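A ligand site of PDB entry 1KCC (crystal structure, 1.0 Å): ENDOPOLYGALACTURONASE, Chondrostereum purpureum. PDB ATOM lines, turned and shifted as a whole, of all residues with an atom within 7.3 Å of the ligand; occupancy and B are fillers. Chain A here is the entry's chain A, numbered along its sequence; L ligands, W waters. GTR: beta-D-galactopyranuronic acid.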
ATOM      1  N   GLY A  87       8.892 -18.076 -21.432  1.00  0.00           N
ATOM      2  CA  GLY A  87       8.633 -19.477 -21.651  1.00  0.00           C
ATOM      3  C   GLY A  87       9.860 -20.319 -21.918  1.00  0.00           C
ATOM      4  O   GLY A  87       9.708 -21.537 -22.008  1.00  0.00           O
ATOM      5  N   LYS A  88      11.061 -19.717 -22.035  1.00  0.00           N
ATOM      6  CA  LYS A  88      12.260 -20.475 -22.438  1.00  0.00           C
ATOM      7  C   LYS A  88      13.288 -20.528 -21.351  1.00  0.00           C
ATOM      8  O   LYS A  88      14.280 -21.283 -21.471  1.00  0.00           O
ATOM      9  CB  LYS A  88      12.855 -19.906 -23.728  1.00  0.00           C
ATOM     10  CG  LYS A  88      11.844 -19.984 -24.915  1.00  0.00           C
ATOM     11  CD  LYS A  88      12.472 -19.422 -26.169  1.00  0.00           C
ATOM     12  CE  LYS A  88      11.605 -19.687 -27.418  1.00  0.00           C
ATOM     13  NZ  LYS A  88      12.413 -19.313 -28.676  1.00  0.00           N
ATOM     14  N   GLY A  89      13.116 -19.770 -20.266  1.00  0.00           N
ATOM     15  CA  GLY A  89      14.083 -19.904 -19.148  1.00  0.00           C
ATOM     16  C   GLY A  89      15.514 -19.674 -19.591  1.00  0.00           C
ATOM     17  O   GLY A  89      15.820 -18.783 -20.390  1.00  0.00           O
ATOM     18  N   THR A  90      16.390 -20.484 -19.020  1.00  0.00           N
ATOM     19  CA  THR A  90      17.807 -20.383 -19.352  1.00  0.00           C
ATOM     20  C   THR A  90      18.206 -21.286 -20.495  1.00  0.00           C
ATOM     21  O   THR A  90      19.383 -21.452 -20.781  1.00  0.00           O
ATOM     22  CB  THR A  90      18.653 -20.593 -18.058  1.00  0.00           C
ATOM     23  OG1 THR A  90      18.276 -21.785 -17.378  1.00  0.00           O
ATOM     24  CG2 THR A  90      18.430 -19.444 -17.082  1.00  0.00           C
ATOM     25  N   ASN A  91      17.200 -21.909 -21.147  1.00  0.00           N
ATOM     26  CA  ASN A  91      17.514 -22.765 -22.268  1.00  0.00           C
ATOM     27  C   ASN A  91      17.673 -22.025 -23.540  1.00  0.00           C
ATOM     28  O   ASN A  91      18.445 -22.490 -24.441  1.00  0.00           O
ATOM     29  CB  ASN A  91      16.412 -23.854 -22.398  1.00  0.00           C
ATOM     30  CG  ASN A  91      16.587 -24.818 -21.197  1.00  0.00           C
ATOM     31  OD1 ASN A  91      17.750 -25.128 -20.785  1.00  0.00           O
ATOM     32  ND2 ASN A  91      15.535 -25.308 -20.624  1.00  0.00           N
ATOM     33  N   GLN A 120      16.729 -18.912 -12.030  1.00  0.00           N
ATOM     34  CA  GLN A 120      17.039 -19.607 -10.767  1.00  0.00           C
ATOM     35  C   GLN A 120      17.147 -18.561  -9.635  1.00  0.00           C
ATOM     36  O   GLN A 120      17.802 -17.510  -9.796  1.00  0.00           O
ATOM     37  CB  GLN A 120      18.342 -20.390 -10.879  1.00  0.00           C
ATOM     38  CG  GLN A 120      18.270 -21.554 -11.885  1.00  0.00           C
ATOM     39  CD  GLN A 120      18.571 -21.168 -13.313  1.00  0.00           C
ATOM     40  OE1 GLN A 120      18.537 -20.011 -13.727  1.00  0.00           O
ATOM     41  NE2 GLN A 120      18.779 -22.187 -14.202  1.00  0.00           N
ATOM     42  N   HIS A 150      10.244 -20.089 -16.090  1.00  0.00           N
ATOM     43  CA  HIS A 150      10.886 -21.366 -16.403  1.00  0.00           C
ATOM     44  C   HIS A 150      12.272 -21.351 -15.777  1.00  0.00           C
ATOM     45  O   HIS A 150      12.914 -20.293 -15.652  1.00  0.00           O
ATOM     46  CB  HIS A 150      10.904 -21.577 -17.902  1.00  0.00           C
ATOM     47  CG  HIS A 150      11.135 -23.027 -18.241  1.00  0.00           C
ATOM     48  ND1 HIS A 150      10.157 -23.989 -18.104  1.00  0.00           N
ATOM     49  CD2 HIS A 150      12.234 -23.647 -18.720  1.00  0.00           C
ATOM     50  CE1 HIS A 150      10.627 -25.180 -18.459  1.00  0.00           C
ATOM     51  NE2 HIS A 150      11.907 -25.002 -18.863  1.00  0.00           N
ATOM     52  N   ASN A 151      12.764 -22.520 -15.384  1.00  0.00           N
ATOM     53  CA  ASN A 151      14.072 -22.624 -14.736  1.00  0.00           C
ATOM     54  C   ASN A 151      14.137 -21.735 -13.475  1.00  0.00           C
ATOM     55  O   ASN A 151      15.213 -21.272 -13.091  1.00  0.00           O
ATOM     56  CB  ASN A 151      15.253 -22.288 -15.667  1.00  0.00           C
ATOM     57  CG  ASN A 151      15.334 -23.264 -16.817  1.00  0.00           C
ATOM     58  OD1 ASN A 151      15.216 -22.849 -17.987  1.00  0.00           O
ATOM     59  ND2 ASN A 151      15.529 -24.554 -16.547  1.00  0.00           N
ATOM     60  N   THR A 152      12.992 -21.610 -12.809  1.00  0.00           N
ATOM     61  CA  THR A 152      12.894 -20.762 -11.585  1.00  0.00           C
ATOM     62  C   THR A 152      13.157 -21.568 -10.307  1.00  0.00           C
ATOM     63  O   THR A 152      12.409 -21.497  -9.345  1.00  0.00           O
ATOM     64  CB  THR A 152      11.520 -20.081 -11.567  1.00  0.00           C
ATOM     65  OG1 THR A 152      10.545 -21.092 -11.932  1.00  0.00           O
ATOM     66  CG2 THR A 152      11.470 -18.904 -12.551  1.00  0.00           C
ATOM     67  N   ASP A 153      14.308 -22.279 -10.311  1.00  0.00           N
ATOM     68  CA  ASP A 153      14.644 -23.114  -9.161  1.00  0.00           C
ATOM     69  C   ASP A 153      14.601 -22.288  -7.866  1.00  0.00           C
ATOM     70  O   ASP A 153      15.054 -21.162  -7.814  1.00  0.00           O
ATOM     71  CB  ASP A 153      16.090 -23.613  -9.275  1.00  0.00           C
ATOM     72  CG  ASP A 153      16.444 -24.418 -10.500  1.00  0.00           C
ATOM     73  OD1 ASP A 153      15.746 -24.283 -11.526  1.00  0.00           O
ATOM     74  OD2 ASP A 153      17.434 -25.184 -10.445  1.00  0.00           O
ATOM     75  N   GLN A 172       8.440 -22.914 -10.987  1.00  0.00           N
ATOM     76  CA  GLN A 172       8.229 -23.678 -12.238  1.00  0.00           C
ATOM     77  C   GLN A 172       9.353 -24.635 -12.509  1.00  0.00           C
ATOM     78  O   GLN A 172       9.441 -25.186 -13.616  1.00  0.00           O
ATOM     79  CB  GLN A 172       8.030 -22.767 -13.447  1.00  0.00           C
ATOM     80  CG  GLN A 172       6.814 -21.825 -13.361  1.00  0.00           C
ATOM     81  CD  GLN A 172       7.069 -20.628 -12.465  1.00  0.00           C
ATOM     82  OE1 GLN A 172       8.149 -19.991 -12.509  1.00  0.00           O
ATOM     83  NE2 GLN A 172       6.067 -20.255 -11.690  1.00  0.00           N
ATOM     84  N   ASP A 173      10.258 -24.876 -11.525  1.00  0.00           N
ATOM     85  CA  ASP A 173      11.308 -25.877 -11.727  1.00  0.00           C
ATOM     86  C   ASP A 173      11.617 -26.478 -10.364  1.00  0.00           C
ATOM     87  O   ASP A 173      10.760 -26.426  -9.444  1.00  0.00           O
ATOM     88  CB  ASP A 173      12.547 -25.271 -12.424  1.00  0.00           C
ATOM     89  CG  ASP A 173      13.373 -26.337 -13.196  1.00  0.00           C
ATOM     90  OD1 ASP A 173      13.293 -26.372 -14.434  1.00  0.00           O
ATOM     91  OD2 ASP A 173      14.088 -27.127 -12.558  1.00  0.00           O
ATOM     92  N   ASP A 174      12.769 -27.101 -10.187  1.00  0.00           N
ATOM     93  CA  ASP A 174      13.067 -27.765  -8.922  1.00  0.00           C
ATOM     94  C   ASP A 174      12.838 -26.829  -7.740  1.00  0.00           C
ATOM     95  O   ASP A 174      13.280 -25.676  -7.751  1.00  0.00           O
ATOM     96  CB  ASP A 174      14.520 -28.278  -8.903  1.00  0.00           C
ATOM     97  CG  ASP A 174      14.682 -29.484  -9.850  1.00  0.00           C
ATOM     98  OD1 ASP A 174      13.780 -30.352  -9.836  1.00  0.00           O
ATOM     99  OD2 ASP A 174      15.756 -29.574 -10.483  1.00  0.00           O
ATOM    100  N   GLY A 194       6.294 -26.523  -9.088  1.00  0.00           N
ATOM    101  CA  GLY A 194       7.564 -26.759  -9.798  1.00  0.00           C
ATOM    102  C   GLY A 194       7.768 -28.224 -10.126  1.00  0.00           C
ATOM    103  O   GLY A 194       6.837 -28.948 -10.529  1.00  0.00           O
ATOM    104  N   HIS A 195       9.037 -28.634 -10.038  1.00  0.00           N
ATOM    105  CA  HIS A 195       9.473 -29.948 -10.470  1.00  0.00           C
ATOM    106  C   HIS A 195       9.908 -30.822  -9.288  1.00  0.00           C
ATOM    107  O   HIS A 195      10.485 -31.887  -9.546  1.00  0.00           O
ATOM    108  CB  HIS A 195      10.590 -29.861 -11.515  1.00  0.00           C
ATOM    109  CG  HIS A 195      10.152 -29.197 -12.817  1.00  0.00           C
ATOM    110  ND1 HIS A 195      10.984 -29.097 -13.915  1.00  0.00           N
ATOM    111  CD2 HIS A 195       8.991 -28.634 -13.186  1.00  0.00           C
ATOM    112  CE1 HIS A 195      10.346 -28.477 -14.884  1.00  0.00           C
ATOM    113  NE2 HIS A 195       9.133 -28.173 -14.466  1.00  0.00           N
ATOM    114  N   GLY A 196       9.573 -30.434  -8.087  1.00  0.00           N
ATOM    115  CA  GLY A 196       9.798 -31.325  -6.918  1.00  0.00           C
ATOM    116  C   GLY A 196      11.145 -31.115  -6.282  1.00  0.00           C
ATOM    117  O   GLY A 196      11.865 -30.128  -6.482  1.00  0.00           O
ATOM    118  N   SER A 198      14.855 -32.266  -5.763  1.00  0.00           N
ATOM    119  CA  SER A 198      15.814 -32.983  -6.596  1.00  0.00           C
ATOM    120  C   SER A 198      17.220 -33.001  -6.014  1.00  0.00           C
ATOM    121  O   SER A 198      17.730 -32.019  -5.460  1.00  0.00           O
ATOM    122  CB  SER A 198      15.894 -32.343  -7.984  1.00  0.00           C
ATOM    123  OG  SER A 198      14.712 -32.605  -8.683  1.00  0.00           O
ATOM    124  N   GLY A 200      20.615 -33.404  -8.141  1.00  0.00           N
ATOM    125  CA  GLY A 200      21.096 -33.324  -9.506  1.00  0.00           C
ATOM    126  C   GLY A 200      20.357 -32.267 -10.339  1.00  0.00           C
ATOM    127  O   GLY A 200      19.579 -31.481  -9.830  1.00  0.00           O
ATOM    128  N   SER A 201      20.631 -32.248 -11.654  1.00  0.00           N
ATOM    129  CA  SER A 201      21.358 -33.325 -12.350  1.00  0.00           C
ATOM    130  C   SER A 201      22.808 -33.362 -11.925  1.00  0.00           C
ATOM    131  O   SER A 201      23.534 -32.331 -11.779  1.00  0.00           O
ATOM    132  CB  SER A 201      21.175 -33.129 -13.884  1.00  0.00           C
ATOM    133  OG  SER A 201      22.068 -32.218 -14.382  1.00  0.00           O
ATOM    134  N   MET A 222       5.609 -31.429 -11.063  1.00  0.00           N
ATOM    135  CA  MET A 222       5.797 -32.404 -12.134  1.00  0.00           C
ATOM    136  C   MET A 222       6.365 -33.726 -11.617  1.00  0.00           C
ATOM    137  O   MET A 222       6.083 -34.798 -12.196  1.00  0.00           O
ATOM    138  CB  MET A 222       6.776 -31.841 -13.199  1.00  0.00           C
ATOM    139  CG  MET A 222       6.067 -30.688 -13.911  1.00  0.00           C
ATOM    140  SD  MET A 222       6.786 -30.387 -15.515  1.00  0.00           S
ATOM    141  CE  MET A 222       8.001 -31.644 -15.544  1.00  0.00           C
ATOM    142  N   TYR A 223       7.181 -33.659 -10.570  1.00  0.00           N
ATOM    143  CA  TYR A 223       7.794 -34.843  -9.941  1.00  0.00           C
ATOM    144  C   TYR A 223       7.670 -34.639  -8.441  1.00  0.00           C
ATOM    145  O   TYR A 223       7.595 -33.490  -7.949  1.00  0.00           O
ATOM    146  CB  TYR A 223       9.265 -34.987 -10.277  1.00  0.00           C
ATOM    147  CG  TYR A 223       9.617 -34.969 -11.764  1.00  0.00           C
ATOM    148  CD1 TYR A 223       9.728 -36.128 -12.515  1.00  0.00           C
ATOM    149  CD2 TYR A 223       9.871 -33.715 -12.359  1.00  0.00           C
ATOM    150  CE1 TYR A 223      10.063 -36.034 -13.831  1.00  0.00           C
ATOM    151  CE2 TYR A 223      10.218 -33.682 -13.710  1.00  0.00           C
ATOM    152  CZ  TYR A 223      10.284 -34.867 -14.447  1.00  0.00           C
ATOM    153  OH  TYR A 223      10.672 -34.787 -15.758  1.00  0.00           O
ATOM    154  N   ARG A 226      13.246 -36.625  -7.006  1.00  0.00           N
ATOM    155  CA  ARG A 226      14.098 -37.152  -8.044  1.00  0.00           C
ATOM    156  C   ARG A 226      15.556 -37.205  -7.601  1.00  0.00           C
ATOM    157  O   ARG A 226      16.034 -36.302  -6.931  1.00  0.00           O
ATOM    158  CB  ARG A 226      14.087 -36.290  -9.305  1.00  0.00           C
ATOM    159  CG  ARG A 226      12.909 -36.499 -10.217  1.00  0.00           C
ATOM    160  CD  ARG A 226      13.313 -35.781 -11.589  1.00  0.00           C
ATOM    161  NE  ARG A 226      13.249 -34.340 -11.288  1.00  0.00           N
ATOM    162  CZ  ARG A 226      13.399 -33.440 -12.300  1.00  0.00           C
ATOM    163  NH1 ARG A 226      13.631 -33.832 -13.544  1.00  0.00           N
ATOM    164  NH2 ARG A 226      13.338 -32.118 -11.995  1.00  0.00           N
ATOM    165  N   LYS A 228      18.667 -37.432 -10.186  1.00  0.00           N
ATOM    166  CA  LYS A 228      18.947 -37.447 -11.613  1.00  0.00           C
ATOM    167  C   LYS A 228      20.429 -37.279 -11.829  1.00  0.00           C
ATOM    168  O   LYS A 228      21.053 -36.359 -11.289  1.00  0.00           O
ATOM    169  CB  LYS A 228      18.170 -36.293 -12.339  1.00  0.00           C
ATOM    170  CG  LYS A 228      17.920 -35.024 -11.561  1.00  0.00           C
ATOM    171  CD  LYS A 228      17.334 -33.884 -12.464  1.00  0.00           C
ATOM    172  CE  LYS A 228      16.895 -32.725 -11.527  1.00  0.00           C
ATOM    173  NZ  LYS A 228      16.547 -31.516 -12.322  1.00  0.00           N
ATOM    174  N   TYR A 262      19.547 -38.956 -17.443  1.00  0.00           N
ATOM    175  CA  TYR A 262      19.233 -37.539 -17.670  1.00  0.00           C
ATOM    176  C   TYR A 262      20.015 -37.017 -18.844  1.00  0.00           C
ATOM    177  O   TYR A 262      21.210 -37.306 -18.978  1.00  0.00           O
ATOM    178  CB  TYR A 262      19.572 -36.768 -16.378  1.00  0.00           C
ATOM    179  CG  TYR A 262      18.962 -35.364 -16.403  1.00  0.00           C
ATOM    180  CD1 TYR A 262      17.641 -35.160 -15.955  1.00  0.00           C
ATOM    181  CD2 TYR A 262      19.687 -34.306 -16.841  1.00  0.00           C
ATOM    182  CE1 TYR A 262      17.071 -33.895 -15.960  1.00  0.00           C
ATOM    183  CE2 TYR A 262      19.126 -33.002 -16.861  1.00  0.00           C
ATOM    184  CZ  TYR A 262      17.810 -32.843 -16.415  1.00  0.00           C
ATOM    185  OH  TYR A 262      17.270 -31.559 -16.423  1.00  0.00           O
ATOM    186  N   PRO A 263      19.486 -36.097 -19.651  1.00  0.00           N
ATOM    187  CA  PRO A 263      18.231 -35.338 -19.513  1.00  0.00           C
ATOM    188  C   PRO A 263      16.966 -36.080 -19.897  1.00  0.00           C
ATOM    189  O   PRO A 263      15.877 -35.535 -19.793  1.00  0.00           O
ATOM    190  CB  PRO A 263      18.456 -34.144 -20.457  1.00  0.00           C
ATOM    191  CG  PRO A 263      19.285 -34.700 -21.555  1.00  0.00           C
ATOM    192  CD  PRO A 263      20.238 -35.663 -20.861  1.00  0.00           C
ATOM    193  N   ASP A 265      14.151 -38.982 -18.923  1.00  0.00           N
ATOM    194  CA  ASP A 265      13.738 -39.585 -17.665  1.00  0.00           C
ATOM    195  C   ASP A 265      14.257 -41.034 -17.575  1.00  0.00           C
ATOM    196  O   ASP A 265      14.791 -41.452 -16.536  1.00  0.00           O
ATOM    197  CB  ASP A 265      12.222 -39.574 -17.522  1.00  0.00           C
ATOM    198  CG  ASP A 265      11.606 -38.234 -17.326  1.00  0.00           C
ATOM    199  OD1 ASP A 265      12.140 -37.383 -16.566  1.00  0.00           O
ATOM    200  OD2 ASP A 265      10.563 -37.929 -17.894  1.00  0.00           O
HETATM  201  C1  GTR L   1      12.697 -28.788 -17.879  1.00  0.00           C
HETATM  202  C2  GTR L   1      13.713 -27.681 -18.072  1.00  0.00           C
HETATM  203  C3  GTR L   1      15.059 -28.200 -17.937  1.00  0.00           C
HETATM  204  C4  GTR L   1      15.285 -28.886 -16.554  1.00  0.00           C
HETATM  205  C5  GTR L   1      14.160 -29.932 -16.426  1.00  0.00           C
HETATM  206  C6  GTR L   1      14.191 -30.591 -15.064  1.00  0.00           C
HETATM  207  O1  GTR L   1      11.392 -28.309 -17.988  1.00  0.00           O
HETATM  208  O2  GTR L   1      13.515 -27.093 -19.375  1.00  0.00           O
HETATM  209  O3  GTR L   1      16.035 -27.083 -18.074  1.00  0.00           O
HETATM  210  O4  GTR L   1      15.231 -27.901 -15.500  1.00  0.00           O
HETATM  211  O5  GTR L   1      12.849 -29.333 -16.575  1.00  0.00           O
HETATM  212  O6A GTR L   1      13.312 -30.408 -14.196  1.00  0.00           O
HETATM  213  O6B GTR L   1      15.167 -31.337 -14.883  1.00  0.00           O
HETATM  214  O   HOH W   1      14.239 -28.774 -21.316  1.00  0.00           O
HETATM  215  O   HOH W   2      16.545 -25.253 -13.913  1.00  0.00           O
HETATM  216  O   HOH W   3      13.147 -33.232 -16.589  1.00  0.00           O
HETATM  217  O   HOH W   4      10.991 -31.882 -16.841  1.00  0.00           O
HETATM  218  O   HOH W   5      18.318 -27.660 -17.262  1.00  0.00           O
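Water W4 bridges the side-chain hydroxyl of Tyr 223 and an oxygen (O5) of the ligand.
Water W3 lies within hydrogen-bond range of the side-chain hydroxyl of Tyr 223, the guanidinium group of Arg 226 and an oxygen (O6B) of the ligand.
Water W2 lies within hydrogen-bond range of the side-chain carboxylate (OD1) of Asp 153, the side-chain amide nitrogen (ND2) of Asn 151, an oxygen (O4) of the ligand and the side-chain carboxylate (OD2) of Asp 173.
OD1 of Asp 174 is in salt-bridge range of NH2 of Arg 226, at 2.8 Å.
NE2 of His 195 sits at hydrogen-bond distance from O of Gln 172 (3.1 Å).
OD2 of Asp 174 is in salt-bridge range of NZ of Lys 228 (2.8 Å).
N of His 195 sits at hydrogen-bond distance from O of Asp 173, at 2.9 Å.
The side-chain amide oxygen (OD1) of Asn 151 lies within hydrogen-bond range of the backbone NH (N) of Thr 90 (2.8 Å).
O of Asn 151 sits at hydrogen-bond distance from N of Gln 120, at 3.0 Å.
A ring nitrogen (NE2) of His 195 sits at hydrogen-bond distance from the side-chain sulfur (SD) of Met 222, at 3.4 Å.
The guanidinium group (NE) of Arg 226 is in hydrogen-bond range of the side-chain hydroxyl (OG) of Ser 198 (3.5 Å).
Hydrophobic or aromatic side chains that line the ligand: His 150, His 195 and Tyr 262.
Eight residues have an atom within 4 Å of the ligand: Asn 91, His 150, Asn 151, Asp 173, His 195, Arg 226, Lys 228 and Tyr 262.
The nearest printed residue that does not touch the ligand is Asp 174 (4.4 Å).
A ring nitrogen (NE2) of His 150 is in hydrogen-bond range of an oxygen (O2) of the ligand (2.7 Å).
The side-chain hydroxyl (OH) of Tyr 262 is in hydrogen-bond range of an oxygen (O6B) of the ligand (2.6 Å).
O4 of the ligand is in hydrogen-bond range of OD1 of Asp 173 (2.7 Å).
O2 of the ligand lies within hydrogen-bond range of ND2 of Asn 91 (3.0 Å).
A ring nitrogen (ND1) of His 195 sits at hydrogen-bond distance from an oxygen (O6A) of the ligand, 2.7 Å away.
The guanidinium group (NH2) of Arg 226 is in salt-bridge range of an oxygen (O6A) of the ligand (2.8 Å).
NZ of Lys 228 is in salt-bridge range of O6B of the ligand (2.9 Å).
An oxygen (O3) of the ligand lies within hydrogen-bond range of the side-chain amide nitrogen (ND2) of Asn 151.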
